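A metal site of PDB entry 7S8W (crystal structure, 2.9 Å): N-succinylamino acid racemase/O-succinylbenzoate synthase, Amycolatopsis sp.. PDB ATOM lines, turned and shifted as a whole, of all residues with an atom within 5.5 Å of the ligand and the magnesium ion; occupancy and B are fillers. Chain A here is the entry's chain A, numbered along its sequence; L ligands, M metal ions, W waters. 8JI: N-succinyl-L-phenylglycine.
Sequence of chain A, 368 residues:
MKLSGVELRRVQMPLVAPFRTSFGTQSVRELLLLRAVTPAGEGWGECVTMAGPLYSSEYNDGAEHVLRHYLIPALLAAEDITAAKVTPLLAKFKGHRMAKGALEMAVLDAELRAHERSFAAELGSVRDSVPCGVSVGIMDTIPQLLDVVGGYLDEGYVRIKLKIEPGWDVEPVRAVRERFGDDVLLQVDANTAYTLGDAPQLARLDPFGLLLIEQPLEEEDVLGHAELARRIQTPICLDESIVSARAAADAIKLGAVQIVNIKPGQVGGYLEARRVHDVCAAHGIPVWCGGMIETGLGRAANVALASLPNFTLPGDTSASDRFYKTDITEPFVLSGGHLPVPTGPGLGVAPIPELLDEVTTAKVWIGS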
ATOM      1  N   PHE A  19     -13.706  33.908   8.702  1.00  0.00           N
ATOM      2  CA  PHE A  19     -14.370  33.085   7.697  1.00  0.00           C
ATOM      3  C   PHE A  19     -14.948  34.017   6.645  1.00  0.00           C
ATOM      4  O   PHE A  19     -15.860  34.788   6.938  1.00  0.00           O
ATOM      5  CB  PHE A  19     -15.452  32.224   8.362  1.00  0.00           C
ATOM      6  CG  PHE A  19     -16.138  31.276   7.434  1.00  0.00           C
ATOM      7  CD1 PHE A  19     -15.417  30.283   6.785  1.00  0.00           C
ATOM      8  CD2 PHE A  19     -17.503  31.345   7.221  1.00  0.00           C
ATOM      9  CE1 PHE A  19     -16.036  29.406   5.921  1.00  0.00           C
ATOM     10  CE2 PHE A  19     -18.125  30.466   6.370  1.00  0.00           C
ATOM     11  CZ  PHE A  19     -17.393  29.492   5.719  1.00  0.00           C
ATOM     12  N   THR A  21     -16.795  34.891   2.991  1.00  0.00           N
ATOM     13  CA  THR A  21     -17.698  34.449   1.945  1.00  0.00           C
ATOM     14  C   THR A  21     -17.964  35.622   1.015  1.00  0.00           C
ATOM     15  O   THR A  21     -17.583  36.758   1.298  1.00  0.00           O
ATOM     16  CB  THR A  21     -19.033  33.951   2.510  1.00  0.00           C
ATOM     17  OG1 THR A  21     -19.709  35.056   3.136  1.00  0.00           O
ATOM     18  CG2 THR A  21     -18.811  32.838   3.535  1.00  0.00           C
ATOM     19  N   PHE A  23     -20.223  37.467   0.668  1.00  0.00           N
ATOM     20  CA  PHE A  23     -20.969  38.571   1.241  1.00  0.00           C
ATOM     21  C   PHE A  23     -20.350  39.110   2.527  1.00  0.00           C
ATOM     22  O   PHE A  23     -20.975  39.931   3.198  1.00  0.00           O
ATOM     23  CB  PHE A  23     -22.426  38.165   1.531  1.00  0.00           C
ATOM     24  CG  PHE A  23     -22.568  37.069   2.568  1.00  0.00           C
ATOM     25  CD1 PHE A  23     -22.505  37.353   3.925  1.00  0.00           C
ATOM     26  CD2 PHE A  23     -22.747  35.761   2.176  1.00  0.00           C
ATOM     27  CE1 PHE A  23     -22.614  36.343   4.865  1.00  0.00           C
ATOM     28  CE2 PHE A  23     -22.871  34.744   3.113  1.00  0.00           C
ATOM     29  CZ  PHE A  23     -22.804  35.040   4.458  1.00  0.00           C
ATOM     30  N   GLN A  26     -16.659  36.916   8.480  1.00  0.00           N
ATOM     31  CA  GLN A  26     -17.168  36.750   9.815  1.00  0.00           C
ATOM     32  C   GLN A  26     -16.029  36.386  10.708  1.00  0.00           C
ATOM     33  O   GLN A  26     -15.227  35.549  10.359  1.00  0.00           O
ATOM     34  CB  GLN A  26     -18.168  35.622   9.831  1.00  0.00           C
ATOM     35  CG  GLN A  26     -19.606  36.045   9.644  1.00  0.00           C
ATOM     36  CD  GLN A  26     -20.552  35.243  10.494  1.00  0.00           C
ATOM     37  OE1 GLN A  26     -20.740  35.525  11.671  1.00  0.00           O
ATOM     38  NE2 GLN A  26     -21.134  34.215   9.906  1.00  0.00           N
ATOM     39  N   MET A  50     -27.796  35.798  11.611  1.00  0.00           N
ATOM     40  CA  MET A  50     -26.584  36.534  11.922  1.00  0.00           C
ATOM     41  C   MET A  50     -26.960  37.934  12.398  1.00  0.00           C
ATOM     42  O   MET A  50     -28.140  38.277  12.547  1.00  0.00           O
ATOM     43  CB  MET A  50     -25.640  36.623  10.721  1.00  0.00           C
ATOM     44  CG  MET A  50     -25.661  35.422   9.825  1.00  0.00           C
ATOM     45  SD  MET A  50     -24.065  35.255   8.996  1.00  0.00           S
ATOM     46  CE  MET A  50     -24.018  36.787   8.061  1.00  0.00           C
ATOM     47  N   TYR A  55     -27.059  37.492   4.763  1.00  0.00           N
ATOM     48  CA  TYR A  55     -27.261  36.174   4.174  1.00  0.00           C
ATOM     49  C   TYR A  55     -28.713  35.968   3.743  1.00  0.00           C
ATOM     50  O   TYR A  55     -28.976  35.376   2.688  1.00  0.00           O
ATOM     51  CB  TYR A  55     -26.830  35.098   5.171  1.00  0.00           C
ATOM     52  CG  TYR A  55     -27.203  33.684   4.779  1.00  0.00           C
ATOM     53  CD1 TYR A  55     -28.415  33.138   5.187  1.00  0.00           C
ATOM     54  CD2 TYR A  55     -26.343  32.893   4.046  1.00  0.00           C
ATOM     55  CE1 TYR A  55     -28.772  31.858   4.835  1.00  0.00           C
ATOM     56  CE2 TYR A  55     -26.685  31.603   3.681  1.00  0.00           C
ATOM     57  CZ  TYR A  55     -27.903  31.090   4.079  1.00  0.00           C
ATOM     58  OH  TYR A  55     -28.248  29.798   3.728  1.00  0.00           O
ATOM     59  N   SER A 135     -15.780  23.458   5.442  1.00  0.00           N
ATOM     60  CA  SER A 135     -16.040  24.608   4.576  1.00  0.00           C
ATOM     61  C   SER A 135     -14.930  25.632   4.802  1.00  0.00           C
ATOM     62  O   SER A 135     -14.772  26.145   5.916  1.00  0.00           O
ATOM     63  CB  SER A 135     -17.412  25.193   4.884  1.00  0.00           C
ATOM     64  OG  SER A 135     -17.653  26.369   4.136  1.00  0.00           O
ATOM     65  N   LYS A 161     -14.841  21.947   0.931  1.00  0.00           N
ATOM     66  CA  LYS A 161     -15.774  22.854   0.266  1.00  0.00           C
ATOM     67  C   LYS A 161     -15.133  24.227   0.249  1.00  0.00           C
ATOM     68  O   LYS A 161     -14.655  24.700   1.287  1.00  0.00           O
ATOM     69  CB  LYS A 161     -17.122  22.881   1.002  1.00  0.00           C
ATOM     70  CG  LYS A 161     -17.928  24.162   0.866  1.00  0.00           C
ATOM     71  CD  LYS A 161     -19.248  24.028   1.611  1.00  0.00           C
ATOM     72  CE  LYS A 161     -19.977  25.361   1.735  1.00  0.00           C
ATOM     73  NZ  LYS A 161     -21.385  25.170   2.202  1.00  0.00           N
ATOM     74  N   LYS A 163     -15.440  28.241  -0.507  1.00  0.00           N
ATOM     75  CA  LYS A 163     -16.265  29.386  -0.830  1.00  0.00           C
ATOM     76  C   LYS A 163     -15.645  30.134  -2.010  1.00  0.00           C
ATOM     77  O   LYS A 163     -14.439  30.436  -2.005  1.00  0.00           O
ATOM     78  CB  LYS A 163     -16.408  30.292   0.385  1.00  0.00           C
ATOM     79  CG  LYS A 163     -17.142  29.604   1.498  1.00  0.00           C
ATOM     80  CD  LYS A 163     -18.623  29.609   1.219  1.00  0.00           C
ATOM     81  CE  LYS A 163     -19.375  29.290   2.461  1.00  0.00           C
ATOM     82  NZ  LYS A 163     -20.589  30.121   2.551  1.00  0.00           N
ATOM     83  N   ASP A 189     -18.933  26.798  -3.161  1.00  0.00           N
ATOM     84  CA  ASP A 189     -20.156  27.485  -2.737  1.00  0.00           C
ATOM     85  C   ASP A 189     -19.982  28.976  -3.028  1.00  0.00           C
ATOM     86  O   ASP A 189     -18.983  29.569  -2.618  1.00  0.00           O
ATOM     87  CB  ASP A 189     -20.416  27.243  -1.243  1.00  0.00           C
ATOM     88  CG  ASP A 189     -21.781  27.745  -0.778  1.00  0.00           C
ATOM     89  OD1 ASP A 189     -22.482  28.437  -1.559  1.00  0.00           O
ATOM     90  OD2 ASP A 189     -22.153  27.470   0.386  1.00  0.00           O
ATOM     91  N   ASN A 191     -22.704  31.477  -2.710  1.00  0.00           N
ATOM     92  CA  ASN A 191     -23.604  32.347  -1.930  1.00  0.00           C
ATOM     93  C   ASN A 191     -24.249  33.428  -2.796  1.00  0.00           C
ATOM     94  O   ASN A 191     -24.275  34.607  -2.442  1.00  0.00           O
ATOM     95  CB  ASN A 191     -22.858  32.959  -0.744  1.00  0.00           C
ATOM     96  CG  ASN A 191     -22.708  31.986   0.406  1.00  0.00           C
ATOM     97  OD1 ASN A 191     -21.601  31.720   0.868  1.00  0.00           O
ATOM     98  ND2 ASN A 191     -23.827  31.437   0.863  1.00  0.00           N
ATOM     99  N   GLU A 214     -22.586  25.109  -5.274  1.00  0.00           N
ATOM    100  CA  GLU A 214     -23.639  25.455  -4.334  1.00  0.00           C
ATOM    101  C   GLU A 214     -24.111  26.889  -4.548  1.00  0.00           C
ATOM    102  O   GLU A 214     -23.307  27.821  -4.529  1.00  0.00           O
ATOM    103  CB  GLU A 214     -23.134  25.285  -2.917  1.00  0.00           C
ATOM    104  CG  GLU A 214     -24.217  25.094  -1.888  1.00  0.00           C
ATOM    105  CD  GLU A 214     -23.627  25.001  -0.506  1.00  0.00           C
ATOM    106  OE1 GLU A 214     -22.527  24.403  -0.393  1.00  0.00           O
ATOM    107  OE2 GLU A 214     -24.247  25.531   0.449  1.00  0.00           O
ATOM    108  N   ASP A 239     -29.005  25.908  -1.922  1.00  0.00           N
ATOM    109  CA  ASP A 239     -28.913  26.151  -0.485  1.00  0.00           C
ATOM    110  C   ASP A 239     -29.915  27.218  -0.061  1.00  0.00           C
ATOM    111  O   ASP A 239     -30.983  26.891   0.488  1.00  0.00           O
ATOM    112  CB  ASP A 239     -27.488  26.565  -0.099  1.00  0.00           C
ATOM    113  CG  ASP A 239     -27.292  26.771   1.407  1.00  0.00           C
ATOM    114  OD1 ASP A 239     -28.240  26.564   2.207  1.00  0.00           O
ATOM    115  OD2 ASP A 239     -26.163  27.133   1.800  1.00  0.00           O
ATOM    116  N   GLU A 240     -29.577  28.484  -0.316  1.00  0.00           N
ATOM    117  CA  GLU A 240     -30.431  29.608   0.076  1.00  0.00           C
ATOM    118  C   GLU A 240     -31.845  29.465  -0.498  1.00  0.00           C
ATOM    119  O   GLU A 240     -32.800  29.988   0.097  1.00  0.00           O
ATOM    120  CB  GLU A 240     -29.822  30.921  -0.405  1.00  0.00           C
ATOM    121  CG  GLU A 240     -28.730  31.569   0.451  1.00  0.00           C
ATOM    122  CD  GLU A 240     -27.314  31.078   0.153  1.00  0.00           C
ATOM    123  OE1 GLU A 240     -27.129  29.966  -0.398  1.00  0.00           O
ATOM    124  OE2 GLU A 240     -26.368  31.862   0.407  1.00  0.00           O
ATOM    125  N   ASN A 261     -28.781  20.990  -0.262  1.00  0.00           N
ATOM    126  CA  ASN A 261     -28.216  21.303   1.056  1.00  0.00           C
ATOM    127  C   ASN A 261     -29.377  21.614   1.996  1.00  0.00           C
ATOM    128  O   ASN A 261     -30.098  22.607   1.795  1.00  0.00           O
ATOM    129  CB  ASN A 261     -27.254  22.492   0.909  1.00  0.00           C
ATOM    130  CG  ASN A 261     -26.700  23.010   2.243  1.00  0.00           C
ATOM    131  OD1 ASN A 261     -27.150  22.658   3.326  1.00  0.00           O
ATOM    132  ND2 ASN A 261     -25.707  23.879   2.133  1.00  0.00           N
ATOM    133  N   LYS A 263     -30.432  23.022   5.373  1.00  0.00           N
ATOM    134  CA  LYS A 263     -30.151  23.797   6.579  1.00  0.00           C
ATOM    135  C   LYS A 263     -31.396  23.869   7.433  1.00  0.00           C
ATOM    136  O   LYS A 263     -32.347  24.587   7.071  1.00  0.00           O
ATOM    137  CB  LYS A 263     -29.659  25.208   6.264  1.00  0.00           C
ATOM    138  CG  LYS A 263     -28.258  25.227   5.789  1.00  0.00           C
ATOM    139  CD  LYS A 263     -27.972  26.647   5.415  1.00  0.00           C
ATOM    140  CE  LYS A 263     -26.556  26.810   4.923  1.00  0.00           C
ATOM    141  NZ  LYS A 263     -26.323  28.215   4.506  1.00  0.00           N
ATOM    142  N   GLY A 290     -26.323  21.209   6.122  1.00  0.00           N
ATOM    143  CA  GLY A 290     -25.640  22.479   6.024  1.00  0.00           C
ATOM    144  C   GLY A 290     -25.311  23.066   7.378  1.00  0.00           C
ATOM    145  O   GLY A 290     -25.980  22.801   8.384  1.00  0.00           O
ATOM    146  N   GLY A 291     -24.262  23.869   7.408  1.00  0.00           N
ATOM    147  CA  GLY A 291     -23.848  24.485   8.654  1.00  0.00           C
ATOM    148  C   GLY A 291     -24.103  25.973   8.694  1.00  0.00           C
ATOM    149  O   GLY A 291     -24.277  26.608   7.660  1.00  0.00           O
ATOM    150  N   MET A 292     -24.170  26.519   9.904  1.00  0.00           N
ATOM    151  CA  MET A 292     -24.280  27.958  10.092  1.00  0.00           C
ATOM    152  C   MET A 292     -23.363  28.411  11.231  1.00  0.00           C
ATOM    153  O   MET A 292     -23.675  29.388  11.937  1.00  0.00           O
ATOM    154  CB  MET A 292     -25.730  28.388  10.359  1.00  0.00           C
ATOM    155  CG  MET A 292     -26.683  28.216   9.177  1.00  0.00           C
ATOM    156  SD  MET A 292     -26.333  29.259   7.730  1.00  0.00           S
ATOM    157  CE  MET A 292     -27.585  30.519   7.918  1.00  0.00           C
ATOM    158  N   ILE A 293     -22.222  27.744  11.408  1.00  0.00           N
ATOM    159  CA  ILE A 293     -21.280  28.021  12.480  1.00  0.00           C
ATOM    160  C   ILE A 293     -22.054  27.989  13.793  1.00  0.00           C
ATOM    161  O   ILE A 293     -22.041  28.960  14.555  1.00  0.00           O
ATOM    162  CB  ILE A 293     -20.553  29.365  12.286  1.00  0.00           C
ATOM    163  CG1 ILE A 293     -20.209  29.602  10.809  1.00  0.00           C
ATOM    164  CG2 ILE A 293     -19.258  29.400  13.080  1.00  0.00           C
ATOM    165  CD1 ILE A 293     -19.579  30.950  10.558  1.00  0.00           C
ATOM    166  N   GLU A 294     -22.756  26.888  14.040  1.00  0.00           N
ATOM    167  CA  GLU A 294     -23.581  26.796  15.223  1.00  0.00           C
ATOM    168  C   GLU A 294     -22.745  26.382  16.437  1.00  0.00           C
ATOM    169  O   GLU A 294     -21.607  25.916  16.317  1.00  0.00           O
ATOM    170  CB  GLU A 294     -24.712  25.778  15.037  1.00  0.00           C
ATOM    171  CG  GLU A 294     -25.766  26.146  14.002  1.00  0.00           C
ATOM    172  CD  GLU A 294     -25.711  25.227  12.816  1.00  0.00           C
ATOM    173  OE1 GLU A 294     -24.574  24.890  12.402  1.00  0.00           O
ATOM    174  OE2 GLU A 294     -26.771  24.829  12.293  1.00  0.00           O
ATOM    175  N   ARG A 299     -25.101  22.031  16.512  1.00  0.00           N
ATOM    176  CA  ARG A 299     -24.213  21.021  15.933  1.00  0.00           C
ATOM    177  C   ARG A 299     -24.693  19.615  16.267  1.00  0.00           C
ATOM    178  O   ARG A 299     -24.614  18.708  15.425  1.00  0.00           O
ATOM    179  CB  ARG A 299     -22.777  21.230  16.413  1.00  0.00           C
ATOM    180  CG  ARG A 299     -21.757  20.370  15.704  1.00  0.00           C
ATOM    181  CD  ARG A 299     -20.340  20.926  15.840  1.00  0.00           C
ATOM    182  NE  ARG A 299     -20.283  22.348  15.520  1.00  0.00           N
ATOM    183  CZ  ARG A 299     -20.155  22.834  14.293  1.00  0.00           C
ATOM    184  NH1 ARG A 299     -20.075  22.006  13.253  1.00  0.00           N
ATOM    185  NH2 ARG A 299     -20.115  24.139  14.111  1.00  0.00           N
ATOM    186  N   ASP A 316     -21.580  19.727   6.192  1.00  0.00           N
ATOM    187  CA  ASP A 316     -20.823  20.773   6.879  1.00  0.00           C
ATOM    188  C   ASP A 316     -20.972  20.587   8.377  1.00  0.00           C
ATOM    189  O   ASP A 316     -21.289  21.527   9.113  1.00  0.00           O
ATOM    190  CB  ASP A 316     -21.325  22.166   6.476  1.00  0.00           C
ATOM    191  CG  ASP A 316     -20.856  22.594   5.094  1.00  0.00           C
ATOM    192  OD1 ASP A 316     -19.883  21.994   4.564  1.00  0.00           O
ATOM    193  OD2 ASP A 316     -21.474  23.531   4.525  1.00  0.00           O
ATOM    194  N   THR A 317     -20.781  19.351   8.834  1.00  0.00           N
ATOM    195  CA  THR A 317     -20.855  19.006  10.249  1.00  0.00           C
ATOM    196  C   THR A 317     -19.434  18.833  10.802  1.00  0.00           C
ATOM    197  O   THR A 317     -19.034  17.758  11.228  1.00  0.00           O
ATOM    198  CB  THR A 317     -21.705  17.752  10.438  1.00  0.00           C
ATOM    199  OG1 THR A 317     -21.313  16.742   9.473  1.00  0.00           O
ATOM    200  CG2 THR A 317     -23.180  18.071  10.234  1.00  0.00           C
ATOM    201  N   SER A 318     -18.698  19.942  10.806  1.00  0.00           N
ATOM    202  CA  SER A 318     -17.311  19.918  11.252  1.00  0.00           C
ATOM    203  C   SER A 318     -17.230  19.777  12.771  1.00  0.00           C
ATOM    204  O   SER A 318     -18.231  19.858  13.504  1.00  0.00           O
ATOM    205  CB  SER A 318     -16.578  21.195  10.814  1.00  0.00           C
ATOM    206  OG  SER A 318     -16.443  21.273   9.405  1.00  0.00           O
ATOM    207  N   PHE A 323     -14.004  25.977  14.573  1.00  0.00           N
ATOM    208  CA  PHE A 323     -14.631  27.277  14.742  1.00  0.00           C
ATOM    209  C   PHE A 323     -14.373  27.834  16.135  1.00  0.00           C
ATOM    210  O   PHE A 323     -14.083  29.024  16.260  1.00  0.00           O
ATOM    211  CB  PHE A 323     -16.140  27.359  14.455  1.00  0.00           C
ATOM    212  CG  PHE A 323     -16.473  27.339  12.994  1.00  0.00           C
ATOM    213  CD1 PHE A 323     -15.987  28.317  12.153  1.00  0.00           C
ATOM    214  CD2 PHE A 323     -17.288  26.341  12.471  1.00  0.00           C
ATOM    215  CE1 PHE A 323     -16.300  28.306  10.793  1.00  0.00           C
ATOM    216  CE2 PHE A 323     -17.601  26.315  11.130  1.00  0.00           C
ATOM    217  CZ  PHE A 323     -17.113  27.304  10.291  1.00  0.00           C
HETATM  218  C15 8JI L   1     -20.081  26.492   7.766  1.00  0.00           C
HETATM  219  C01 8JI L   1     -22.371  32.304   6.863  1.00  0.00           C
HETATM  220  C02 8JI L   1     -21.439  31.286   6.930  1.00  0.00           C
HETATM  221  C03 8JI L   1     -21.722  30.054   6.382  1.00  0.00           C
HETATM  222  C04 8JI L   1     -22.943  29.850   5.774  1.00  0.00           C
HETATM  223  C05 8JI L   1     -23.878  30.865   5.721  1.00  0.00           C
HETATM  224  C06 8JI L   1     -23.596  32.097   6.269  1.00  0.00           C
HETATM  225  C07 8JI L   1     -23.261  28.464   5.194  1.00  0.00           C
HETATM  226  C08 8JI L   1     -23.325  28.432   3.650  1.00  0.00           C
HETATM  227  C12 8JI L   1     -21.090  27.032   5.545  1.00  0.00           C
HETATM  228  C14 8JI L   1     -20.484  25.937   6.408  1.00  0.00           C
HETATM  229  C16 8JI L   1     -20.161  25.455   8.877  1.00  0.00           C
HETATM  230  N11 8JI L   1     -22.442  27.441   5.851  1.00  0.00           N
HETATM  231  O09 8JI L   1     -23.371  29.534   3.035  1.00  0.00           O
HETATM  232  O10 8JI L   1     -23.385  27.353   3.000  1.00  0.00           O
HETATM  233  O13 8JI L   1     -20.477  27.520   4.652  1.00  0.00           O
HETATM  234  O17 8JI L   1     -20.929  25.663   9.850  1.00  0.00           O
HETATM  235  O18 8JI L   1     -19.466  24.412   8.823  1.00  0.00           O
HETATM  236 MG    MG M   1     -24.123  27.452   1.433  1.00  0.00          MG
HETATM  237  O   HOH W   1     -23.768  32.578   9.439  1.00  0.00           O
HETATM  238  O   HOH W   2     -23.754  25.099   4.187  1.00  0.00           O
HETATM  239  O   HOH W   3     -21.981  24.124  11.876  1.00  0.00           O
HETATM  240  O   HOH W   4     -24.827  28.414  -0.426  1.00  0.00           O
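The magnesium ion is bound by an oxygen (O10) of the ligand (1.7 Å), the side-chain carboxylate (OD2) of Asp 239 (2.1 Å), the side-chain carboxylate (OE2) of Glu 214 (2.2 Å), water W4 (2.2 Å) and the side-chain carboxylate (OD2) of Asp 189 (2.2 Å).
The magnesium ion has five donor atoms within binding distance.
Slightly farther from the magnesium ion lies O09 of the ligand (2.7 Å).
Residues that only touch the magnesium ion: Lys 161 (3.6 Å), Asn 261 (3.97 Å) and Lys 263 (3.9 Å).
Of the 26 residues printed, 6 come within 4 Å of the magnesium ion.
The nearest printed residue that does not touch the magnesium ion is Asn 191 (4.04 Å).
Water W4 lies within hydrogen-bond range of the side-chain carboxylate (OD1) of Asp 189 (2.6 Å), the side-chain carboxylate (OE1) of Glu 240 (2.8 Å) and the side-chain amide nitrogen (ND2) of Asn 191 (3.4 Å).
Water W3 lies within hydrogen-bond range of an oxygen (O17) of the ligand, the side-chain carboxylate of Glu 294 and the guanidinium group of Arg 299.
Water W1 bridges SD of Met 50 (2.7 Å) and NE2 of Gln 26 (3.1 Å).
O of Asp 316 sits close to O18 of the ligand.
Residues that only touch the ligand: Phe 19, Phe 323, Phe 23, Tyr 55 and Gln 26.
The nearest printed residue that does not touch the ligand is Met 50 (4.02 Å).
N11 of the ligand is in hydrogen-bond range of O of Gly 291 (2.7 Å).
The side-chain amino group of Lys 163 is in salt-bridge range of an oxygen (O09) of the ligand, 2.9 Å away.
N of Ile 293 is in hydrogen-bond range of O17 of the ligand, 2.9 Å away.
An oxygen (O09) of the ligand sits at hydrogen-bond distance from the side-chain amide nitrogen (ND2) of Asn 191, at 2.9 Å.
O10 of the ligand sits close to NZ of Lys 161.
O13 of the ligand is in hydrogen-bond range of OG of Ser 135 (3.1 Å).
An oxygen (O09) of the ligand lies within salt-bridge range of the side-chain amino group (NZ) of Lys 263.
O17 of the ligand lies within hydrogen-bond range of N of Met 292, 3.4 Å away.
OD1 of Asp 239 lies within salt-bridge range of NZ of Lys 263 (3.4 Å).
The side-chain amino group (NZ) of Lys 163 lies close to the side-chain carboxylate (OD2) of Asp 189, at 3.8 Å.
The side-chain carboxylate of Asp 189 lies within hydrogen-bond range of the backbone NH of Asn 191 (3.3 Å).
OD2 of Asp 189 sits close to NZ of Lys 161, at 3.0 Å.
OE2 of Glu 240 lies within hydrogen-bond range of ND2 of Asn 191 (2.6 Å).
The side-chain sulfur of Met 292 lies within hydrogen-bond range of the side-chain amino group of Lys 263.
OG1 of Thr 21 lies close to N of Phe 23, at 3.5 Å.
The side-chain sulfur (SD) of Met 50 sits at hydrogen-bond distance from the side-chain amide nitrogen (NE2) of Gln 26 (3.2 Å).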
